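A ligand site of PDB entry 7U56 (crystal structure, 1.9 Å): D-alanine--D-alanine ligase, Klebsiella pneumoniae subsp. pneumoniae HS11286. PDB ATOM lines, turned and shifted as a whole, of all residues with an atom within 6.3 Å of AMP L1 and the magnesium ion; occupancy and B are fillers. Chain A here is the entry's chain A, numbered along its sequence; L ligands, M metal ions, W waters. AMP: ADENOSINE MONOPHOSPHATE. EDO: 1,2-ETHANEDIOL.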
ATOM      1  N   LYS A 160     -18.694 -14.932 -24.608  1.00  0.00           N
ATOM      2  CA  LYS A 160     -20.111 -15.204 -24.365  1.00  0.00           C
ATOM      3  C   LYS A 160     -20.690 -16.175 -25.379  1.00  0.00           C
ATOM      4  O   LYS A 160     -21.618 -16.921 -25.045  1.00  0.00           O
ATOM      5  CB  LYS A 160     -20.919 -13.901 -24.343  1.00  0.00           C
ATOM      6  CG  LYS A 160     -20.572 -13.022 -23.121  1.00  0.00           C
ATOM      7  CD  LYS A 160     -21.720 -12.070 -22.751  1.00  0.00           C
ATOM      8  CE  LYS A 160     -21.292 -11.095 -21.671  1.00  0.00           C
ATOM      9  NZ  LYS A 160     -20.105 -10.274 -22.094  1.00  0.00           N
ATOM     10  N   ALA A 175     -30.342 -16.982 -23.585  1.00  0.00           N
ATOM     11  CA  ALA A 175     -31.153 -16.157 -24.474  1.00  0.00           C
ATOM     12  C   ALA A 175     -30.953 -16.616 -25.921  1.00  0.00           C
ATOM     13  O   ALA A 175     -29.808 -16.779 -26.352  1.00  0.00           O
ATOM     14  CB  ALA A 175     -30.810 -14.680 -24.327  1.00  0.00           C
ATOM     15  N   LEU A 201     -33.734  -6.356 -29.229  1.00  0.00           N
ATOM     16  CA  LEU A 201     -32.545  -7.185 -29.269  1.00  0.00           C
ATOM     17  C   LEU A 201     -31.477  -6.572 -28.378  1.00  0.00           C
ATOM     18  O   LEU A 201     -31.453  -5.369 -28.131  1.00  0.00           O
ATOM     19  CB  LEU A 201     -31.985  -7.299 -30.703  1.00  0.00           C
ATOM     20  CG  LEU A 201     -32.959  -7.871 -31.720  1.00  0.00           C
ATOM     21  CD1 LEU A 201     -32.564  -7.527 -33.157  1.00  0.00           C
ATOM     22  CD2 LEU A 201     -33.016  -9.368 -31.505  1.00  0.00           C
ATOM     23  N   PHE A 202     -30.557  -7.411 -27.912  1.00  0.00           N
ATOM     24  CA  PHE A 202     -29.360  -6.928 -27.268  1.00  0.00           C
ATOM     25  C   PHE A 202     -28.172  -7.396 -28.084  1.00  0.00           C
ATOM     26  O   PHE A 202     -28.092  -8.563 -28.487  1.00  0.00           O
ATOM     27  CB  PHE A 202     -29.277  -7.411 -25.817  1.00  0.00           C
ATOM     28  CG  PHE A 202     -30.250  -6.703 -24.945  1.00  0.00           C
ATOM     29  CD1 PHE A 202     -31.568  -7.122 -24.888  1.00  0.00           C
ATOM     30  CD2 PHE A 202     -29.869  -5.579 -24.246  1.00  0.00           C
ATOM     31  CE1 PHE A 202     -32.497  -6.438 -24.119  1.00  0.00           C
ATOM     32  CE2 PHE A 202     -30.790  -4.896 -23.457  1.00  0.00           C
ATOM     33  CZ  PHE A 202     -32.105  -5.327 -23.407  1.00  0.00           C
ATOM     34  N   LYS A 204     -23.981  -7.394 -28.332  1.00  0.00           N
ATOM     35  CA  LYS A 204     -22.795  -7.249 -27.496  1.00  0.00           C
ATOM     36  C   LYS A 204     -21.608  -7.934 -28.143  1.00  0.00           C
ATOM     37  O   LYS A 204     -21.771  -8.923 -28.865  1.00  0.00           O
ATOM     38  CB  LYS A 204     -23.010  -7.805 -26.081  1.00  0.00           C
ATOM     39  CG  LYS A 204     -23.749  -9.116 -25.989  1.00  0.00           C
ATOM     40  CD  LYS A 204     -24.076  -9.511 -24.507  1.00  0.00           C
ATOM     41  CE  LYS A 204     -25.564  -9.479 -24.218  1.00  0.00           C
ATOM     42  NZ  LYS A 204     -25.924  -9.990 -22.839  1.00  0.00           N
ATOM     43  N   SER A 211     -19.253  -3.498 -19.231  1.00  0.00           N
ATOM     44  CA  SER A 211     -20.121  -3.985 -20.314  1.00  0.00           C
ATOM     45  C   SER A 211     -20.043  -3.068 -21.545  1.00  0.00           C
ATOM     46  O   SER A 211     -21.042  -2.500 -22.015  1.00  0.00           O
ATOM     47  CB  SER A 211     -21.566  -4.117 -19.813  1.00  0.00           C
ATOM     48  OG  SER A 211     -21.969  -2.960 -19.106  1.00  0.00           O
ATOM     49  N   VAL A 214     -22.349  -2.924 -25.442  1.00  0.00           N
ATOM     50  CA  VAL A 214     -23.662  -3.560 -25.317  1.00  0.00           C
ATOM     51  C   VAL A 214     -24.744  -2.534 -25.620  1.00  0.00           C
ATOM     52  O   VAL A 214     -24.824  -1.500 -24.947  1.00  0.00           O
ATOM     53  CB  VAL A 214     -23.875  -4.150 -23.913  1.00  0.00           C
ATOM     54  CG1 VAL A 214     -25.289  -4.731 -23.795  1.00  0.00           C
ATOM     55  CG2 VAL A 214     -22.795  -5.192 -23.566  1.00  0.00           C
ATOM     56  N   GLU A 240     -28.821 -11.055 -29.309  1.00  0.00           N
ATOM     57  CA  GLU A 240     -29.685 -11.822 -28.404  1.00  0.00           C
ATOM     58  C   GLU A 240     -31.108 -11.297 -28.385  1.00  0.00           C
ATOM     59  O   GLU A 240     -31.343 -10.092 -28.368  1.00  0.00           O
ATOM     60  CB  GLU A 240     -29.207 -11.750 -26.948  1.00  0.00           C
ATOM     61  CG  GLU A 240     -27.840 -12.234 -26.735  1.00  0.00           C
ATOM     62  CD  GLU A 240     -27.518 -12.395 -25.278  1.00  0.00           C
ATOM     63  OE1 GLU A 240     -28.082 -11.649 -24.444  1.00  0.00           O
ATOM     64  OE2 GLU A 240     -26.695 -13.281 -24.977  1.00  0.00           O
ATOM     65  N   GLN A 241     -32.054 -12.230 -28.302  1.00  0.00           N
ATOM     66  CA  GLN A 241     -33.404 -11.915 -27.887  1.00  0.00           C
ATOM     67  C   GLN A 241     -33.419 -11.229 -26.523  1.00  0.00           C
ATOM     68  O   GLN A 241     -32.753 -11.683 -25.576  1.00  0.00           O
ATOM     69  CB  GLN A 241     -34.213 -13.205 -27.832  1.00  0.00           C
ATOM     70  CG  GLN A 241     -35.653 -13.069 -27.397  1.00  0.00           C
ATOM     71  CD  GLN A 241     -36.335 -14.407 -27.503  1.00  0.00           C
ATOM     72  OE1 GLN A 241     -36.452 -14.979 -28.589  1.00  0.00           O
ATOM     73  NE2 GLN A 241     -36.734 -14.948 -26.368  1.00  0.00           N
ATOM     74  N   GLY A 242     -34.203 -10.159 -26.412  1.00  0.00           N
ATOM     75  CA  GLY A 242     -34.356  -9.508 -25.117  1.00  0.00           C
ATOM     76  C   GLY A 242     -35.175 -10.370 -24.168  1.00  0.00           C
ATOM     77  O   GLY A 242     -36.248 -10.868 -24.524  1.00  0.00           O
ATOM     78  N   ILE A 243     -34.650 -10.560 -22.951  1.00  0.00           N
ATOM     79  CA  ILE A 243     -35.273 -11.375 -21.918  1.00  0.00           C
ATOM     80  C   ILE A 243     -35.996 -10.446 -20.957  1.00  0.00           C
ATOM     81  O   ILE A 243     -35.453  -9.397 -20.592  1.00  0.00           O
ATOM     82  CB  ILE A 243     -34.223 -12.231 -21.173  1.00  0.00           C
ATOM     83  CG1 ILE A 243     -33.435 -13.099 -22.158  1.00  0.00           C
ATOM     84  CG2 ILE A 243     -34.890 -13.115 -20.125  1.00  0.00           C
ATOM     85  CD1 ILE A 243     -34.319 -14.015 -23.008  1.00  0.00           C
ATOM     86  N   LYS A 244     -37.211 -10.802 -20.552  1.00  0.00           N
ATOM     87  CA  LYS A 244     -37.962 -10.021 -19.573  1.00  0.00           C
ATOM     88  C   LYS A 244     -37.802 -10.732 -18.230  1.00  0.00           C
ATOM     89  O   LYS A 244     -38.343 -11.824 -18.037  1.00  0.00           O
ATOM     90  CB  LYS A 244     -39.430  -9.892 -19.975  1.00  0.00           C
ATOM     91  N   GLU A 247     -32.782  -9.482 -12.527  1.00  0.00           N
ATOM     92  CA  GLU A 247     -31.366  -9.746 -12.724  1.00  0.00           C
ATOM     93  C   GLU A 247     -30.779 -10.298 -11.421  1.00  0.00           C
ATOM     94  O   GLU A 247     -30.516  -9.555 -10.467  1.00  0.00           O
ATOM     95  CB  GLU A 247     -30.670  -8.481 -13.214  1.00  0.00           C
ATOM     96  CG  GLU A 247     -31.346  -7.994 -14.511  1.00  0.00           C
ATOM     97  CD  GLU A 247     -30.619  -6.866 -15.231  1.00  0.00           C
ATOM     98  OE1 GLU A 247     -29.456  -6.559 -14.894  1.00  0.00           O
ATOM     99  OE2 GLU A 247     -31.248  -6.273 -16.134  1.00  0.00           O
ATOM    100  N   GLU A 249     -28.023 -12.837  -9.267  1.00  0.00           N
ATOM    101  CA  GLU A 249     -26.625 -13.238  -9.297  1.00  0.00           C
ATOM    102  C   GLU A 249     -26.383 -14.242  -8.180  1.00  0.00           C
ATOM    103  O   GLU A 249     -27.009 -14.163  -7.115  1.00  0.00           O
ATOM    104  CB  GLU A 249     -25.684 -12.027  -9.154  1.00  0.00           C
ATOM    105  CG  GLU A 249     -25.969 -10.935 -10.165  1.00  0.00           C
ATOM    106  CD  GLU A 249     -24.944  -9.831 -10.181  1.00  0.00           C
ATOM    107  OE1 GLU A 249     -24.152  -9.710  -9.210  1.00  0.00           O
ATOM    108  OE2 GLU A 249     -24.920  -9.086 -11.182  1.00  0.00           O
ATOM    109  N   ARG A 319     -19.021 -15.871 -10.416  1.00  0.00           N
ATOM    110  CA  ARG A 319     -20.359 -15.324 -10.194  1.00  0.00           C
ATOM    111  C   ARG A 319     -21.202 -15.613 -11.435  1.00  0.00           C
ATOM    112  O   ARG A 319     -20.803 -15.270 -12.551  1.00  0.00           O
ATOM    113  CB  ARG A 319     -20.296 -13.816  -9.934  1.00  0.00           C
ATOM    114  CG  ARG A 319     -21.632 -13.250  -9.400  1.00  0.00           C
ATOM    115  CD  ARG A 319     -21.618 -11.723  -9.449  1.00  0.00           C
ATOM    116  NE  ARG A 319     -21.683 -11.249 -10.831  1.00  0.00           N
ATOM    117  CZ  ARG A 319     -20.811 -10.397 -11.365  1.00  0.00           C
ATOM    118  NH1 ARG A 319     -19.808  -9.884 -10.660  1.00  0.00           N
ATOM    119  NH2 ARG A 319     -20.945 -10.060 -12.646  1.00  0.00           N
ATOM    120  N   ASP A 321     -24.618 -14.883 -13.455  1.00  0.00           N
ATOM    121  CA  ASP A 321     -25.668 -13.865 -13.612  1.00  0.00           C
ATOM    122  C   ASP A 321     -26.763 -14.427 -14.504  1.00  0.00           C
ATOM    123  O   ASP A 321     -26.490 -14.910 -15.608  1.00  0.00           O
ATOM    124  CB  ASP A 321     -25.137 -12.567 -14.243  1.00  0.00           C
ATOM    125  CG  ASP A 321     -23.939 -11.979 -13.492  1.00  0.00           C
ATOM    126  OD1 ASP A 321     -23.759 -12.331 -12.315  1.00  0.00           O
ATOM    127  OD2 ASP A 321     -23.164 -11.175 -14.099  1.00  0.00           O
ATOM    128  N   PHE A 323     -31.223 -14.144 -15.676  1.00  0.00           N
ATOM    129  CA  PHE A 323     -32.518 -13.484 -15.672  1.00  0.00           C
ATOM    130  C   PHE A 323     -33.537 -14.442 -15.110  1.00  0.00           C
ATOM    131  O   PHE A 323     -33.557 -15.626 -15.479  1.00  0.00           O
ATOM    132  CB  PHE A 323     -32.948 -13.059 -17.084  1.00  0.00           C
ATOM    133  CG  PHE A 323     -32.025 -12.097 -17.736  1.00  0.00           C
ATOM    134  CD1 PHE A 323     -32.041 -10.755 -17.387  1.00  0.00           C
ATOM    135  CD2 PHE A 323     -31.129 -12.524 -18.717  1.00  0.00           C
ATOM    136  CE1 PHE A 323     -31.181  -9.853 -18.001  1.00  0.00           C
ATOM    137  CE2 PHE A 323     -30.279 -11.630 -19.336  1.00  0.00           C
ATOM    138  CZ  PHE A 323     -30.292 -10.299 -18.979  1.00  0.00           C
ATOM    139  N   ASN A 333     -27.103 -15.494 -18.251  1.00  0.00           N
ATOM    140  CA  ASN A 333     -26.540 -14.392 -19.038  1.00  0.00           C
ATOM    141  C   ASN A 333     -25.012 -14.454 -19.166  1.00  0.00           C
ATOM    142  O   ASN A 333     -24.467 -14.200 -20.242  1.00  0.00           O
ATOM    143  CB  ASN A 333     -26.935 -13.056 -18.427  1.00  0.00           C
ATOM    144  CG  ASN A 333     -26.447 -11.878 -19.246  1.00  0.00           C
ATOM    145  OD1 ASN A 333     -26.799 -11.743 -20.414  1.00  0.00           O
ATOM    146  ND2 ASN A 333     -25.615 -11.031 -18.636  1.00  0.00           N
ATOM    147  N   GLU A 334     -24.329 -14.805 -18.084  1.00  0.00           N
ATOM    148  CA  GLU A 334     -22.880 -14.686 -18.037  1.00  0.00           C
ATOM    149  C   GLU A 334     -22.336 -15.466 -16.844  1.00  0.00           C
ATOM    150  O   GLU A 334     -22.994 -15.581 -15.814  1.00  0.00           O
ATOM    151  CB  GLU A 334     -22.450 -13.210 -17.927  1.00  0.00           C
ATOM    152  CG  GLU A 334     -20.968 -12.976 -17.776  1.00  0.00           C
ATOM    153  CD  GLU A 334     -20.587 -11.523 -17.974  1.00  0.00           C
ATOM    154  OE1 GLU A 334     -21.488 -10.656 -17.973  1.00  0.00           O
ATOM    155  OE2 GLU A 334     -19.367 -11.252 -18.146  1.00  0.00           O
ATOM    156  N   ASN A 336     -18.955 -15.077 -14.658  1.00  0.00           N
ATOM    157  CA  ASN A 336     -17.845 -14.159 -14.437  1.00  0.00           C
ATOM    158  C   ASN A 336     -16.798 -14.856 -13.580  1.00  0.00           C
ATOM    159  O   ASN A 336     -17.052 -15.158 -12.417  1.00  0.00           O
ATOM    160  CB  ASN A 336     -18.333 -12.892 -13.756  1.00  0.00           C
ATOM    161  CG  ASN A 336     -19.480 -12.233 -14.479  1.00  0.00           C
ATOM    162  OD1 ASN A 336     -19.279 -11.328 -15.281  1.00  0.00           O
ATOM    163  ND2 ASN A 336     -20.698 -12.697 -14.210  1.00  0.00           N
HETATM  164  P   AMP L   1     -24.364  -7.801 -19.899  1.00  0.00           P
HETATM  165  O1P AMP L   1     -24.922  -8.020 -18.503  1.00  0.00           O
HETATM  166  O2P AMP L   1     -22.963  -7.226 -19.802  1.00  0.00           O
HETATM  167  O3P AMP L   1     -24.534  -9.035 -20.777  1.00  0.00           O
HETATM  168  O5' AMP L   1     -25.344  -6.649 -20.406  1.00  0.00           O
HETATM  169  C5' AMP L   1     -25.565  -5.490 -19.597  1.00  0.00           C
HETATM  170  C4' AMP L   1     -27.027  -5.254 -19.294  1.00  0.00           C
HETATM  171  O4' AMP L   1     -27.792  -5.281 -20.515  1.00  0.00           O
HETATM  172  C3' AMP L   1     -27.715  -6.271 -18.385  1.00  0.00           C
HETATM  173  O3' AMP L   1     -27.508  -6.009 -17.012  1.00  0.00           O
HETATM  174  C2' AMP L   1     -29.170  -6.189 -18.800  1.00  0.00           C
HETATM  175  O2' AMP L   1     -29.825  -5.091 -18.162  1.00  0.00           O
HETATM  176  C1' AMP L   1     -29.058  -5.870 -20.290  1.00  0.00           C
HETATM  177  N9  AMP L   1     -29.128  -7.090 -21.108  1.00  0.00           N
HETATM  178  C8  AMP L   1     -28.101  -7.711 -21.770  1.00  0.00           C
HETATM  179  N7  AMP L   1     -28.472  -8.736 -22.497  1.00  0.00           N
HETATM  180  C5  AMP L   1     -29.844  -8.804 -22.291  1.00  0.00           C
HETATM  181  C6  AMP L   1     -30.839  -9.641 -22.821  1.00  0.00           C
HETATM  182  N6  AMP L   1     -30.617 -10.606 -23.713  1.00  0.00           N
HETATM  183  N1  AMP L   1     -32.116  -9.416 -22.423  1.00  0.00           N
HETATM  184  C2  AMP L   1     -32.364  -8.434 -21.558  1.00  0.00           C
HETATM  185  N3  AMP L   1     -31.501  -7.571 -21.008  1.00  0.00           N
HETATM  186  C4  AMP L   1     -30.249  -7.801 -21.425  1.00  0.00           C
HETATM  187  C1  EDO L   2     -27.821  -9.623 -16.223  1.00  0.00           C
HETATM  188  O1  EDO L   2     -26.522  -9.270 -15.704  1.00  0.00           O
HETATM  189  C2  EDO L   2     -28.301 -10.940 -15.625  1.00  0.00           C
HETATM  190  O2  EDO L   2     -28.377 -10.883 -14.174  1.00  0.00           O
HETATM  191 MG    MG M   1     -24.436  -8.244 -16.447  1.00  0.00          MG
HETATM  192  O   HOH W   1     -23.820 -10.204 -16.594  1.00  0.00           O
HETATM  193  O   HOH W   2     -32.812  -5.319 -19.808  1.00  0.00           O
HETATM  194  O   HOH W   3     -25.372  -6.514 -15.952  1.00  0.00           O
HETATM  195  O   HOH W   4     -23.518  -8.500 -14.306  1.00  0.00           O
HETATM  196  O   HOH W   5     -22.525  -7.523 -17.124  1.00  0.00           O
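The side-chain amino group (NZ) of Lys 204 lies within salt-bridge range of an oxygen (O3P) of AMP L1 (2.7 Å). OE2 of Glu 247 sits at hydrogen-bond distance from O2' of AMP L1. A nitrogen (N1) of AMP L1 is in hydrogen-bond range of the backbone NH of Ile 243, 2.8 Å away. The side-chain carboxylate of Glu 240 lies within hydrogen-bond range of a nitrogen (N6) of AMP L1, 2.8 Å away. O of Gln 241 lies within hydrogen-bond range of N6 of AMP L1 (3.0 Å). The side-chain amide nitrogen (ND2) of Asn 333 is in hydrogen-bond range of an oxygen (O3P) of AMP L1, at 3.1 Å.
NZ of Lys 204 is in salt-bridge range of OE1 of Glu 240 (3.2 Å). NZ of Lys 204 is in hydrogen-bond range of OD1 of Asn 333 (3.1 Å). The backbone NH (N) of Glu 240 sits at hydrogen-bond distance from the backbone carbonyl oxygen (O) of Phe 202 (2.7 Å). The backbone carbonyl oxygen (O) of Asp 321 is in hydrogen-bond range of the backbone NH (N) of Asn 333 (2.8 Å). O of Glu 334 sits at hydrogen-bond distance from N of Asp 321 (2.9 Å). The guanidinium group (NE) of Arg 319 is in salt-bridge range of the side-chain carboxylate (OD1) of Asp 321 (2.8 Å). The side-chain amide nitrogen (ND2) of Asn 336 sits at hydrogen-bond distance from the side-chain carboxylate (OD2) of Asp 321.
Residues that only touch AMP L1: Lys 160 (3.9 Å), Phe 202 (3.2 Å), Ser 211 (3.4 Å), Val 214 (3.9 Å), Gly 242 (3.5 Å) and Phe 323 (3.5 Å). Hydrophobic or aromatic side chains within 4 Å of AMP L1: Phe 202, Val 214, Ile 243 and Phe 323. Within 4 Å of AMP L1: Lys 160, Phe 202, Lys 204, Ser 211, Val 214, Glu 240, Gln 241, Gly 242, Ile 243, Glu 247, Phe 323 and Asn 333.
Asp 321 touches the magnesium ion. Asn 333 touches the magnesium ion (ND2 to MG, 3.7 Å). Of the 20 residues printed, 2 come within 4 Å of the magnesium ion. The nearest printed residue that does not touch the magnesium ion is Glu 334 (4.1 Å).
The magnesium ion is bound by water W3 (2.0 Å), water W1 (2.1 Å), an oxygen (O1P) of AMP L1 (2.1 Å), water W5 (2.2 Å), water W4 (2.3 Å) and an oxygen (O1) of EDO L2 (2.4 Å). The magnesium ion has six donor atoms within binding distance.
Water W4 lies within hydrogen-bond range of the side-chain carboxylate of Asp 321 (2.7 Å), the guanidinium group of Arg 319 (3.4 Å) and the side-chain carboxylate of Glu 249 (3.5 Å). Water W5 bridges O2P of AMP L1 and OE1 of Glu 334. Water W1 lies within hydrogen-bond range of OE1 of Glu 334 (2.7 Å), OD2 of Asp 321 (2.8 Å) and ND2 of Asn 333 (2.8 Å).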
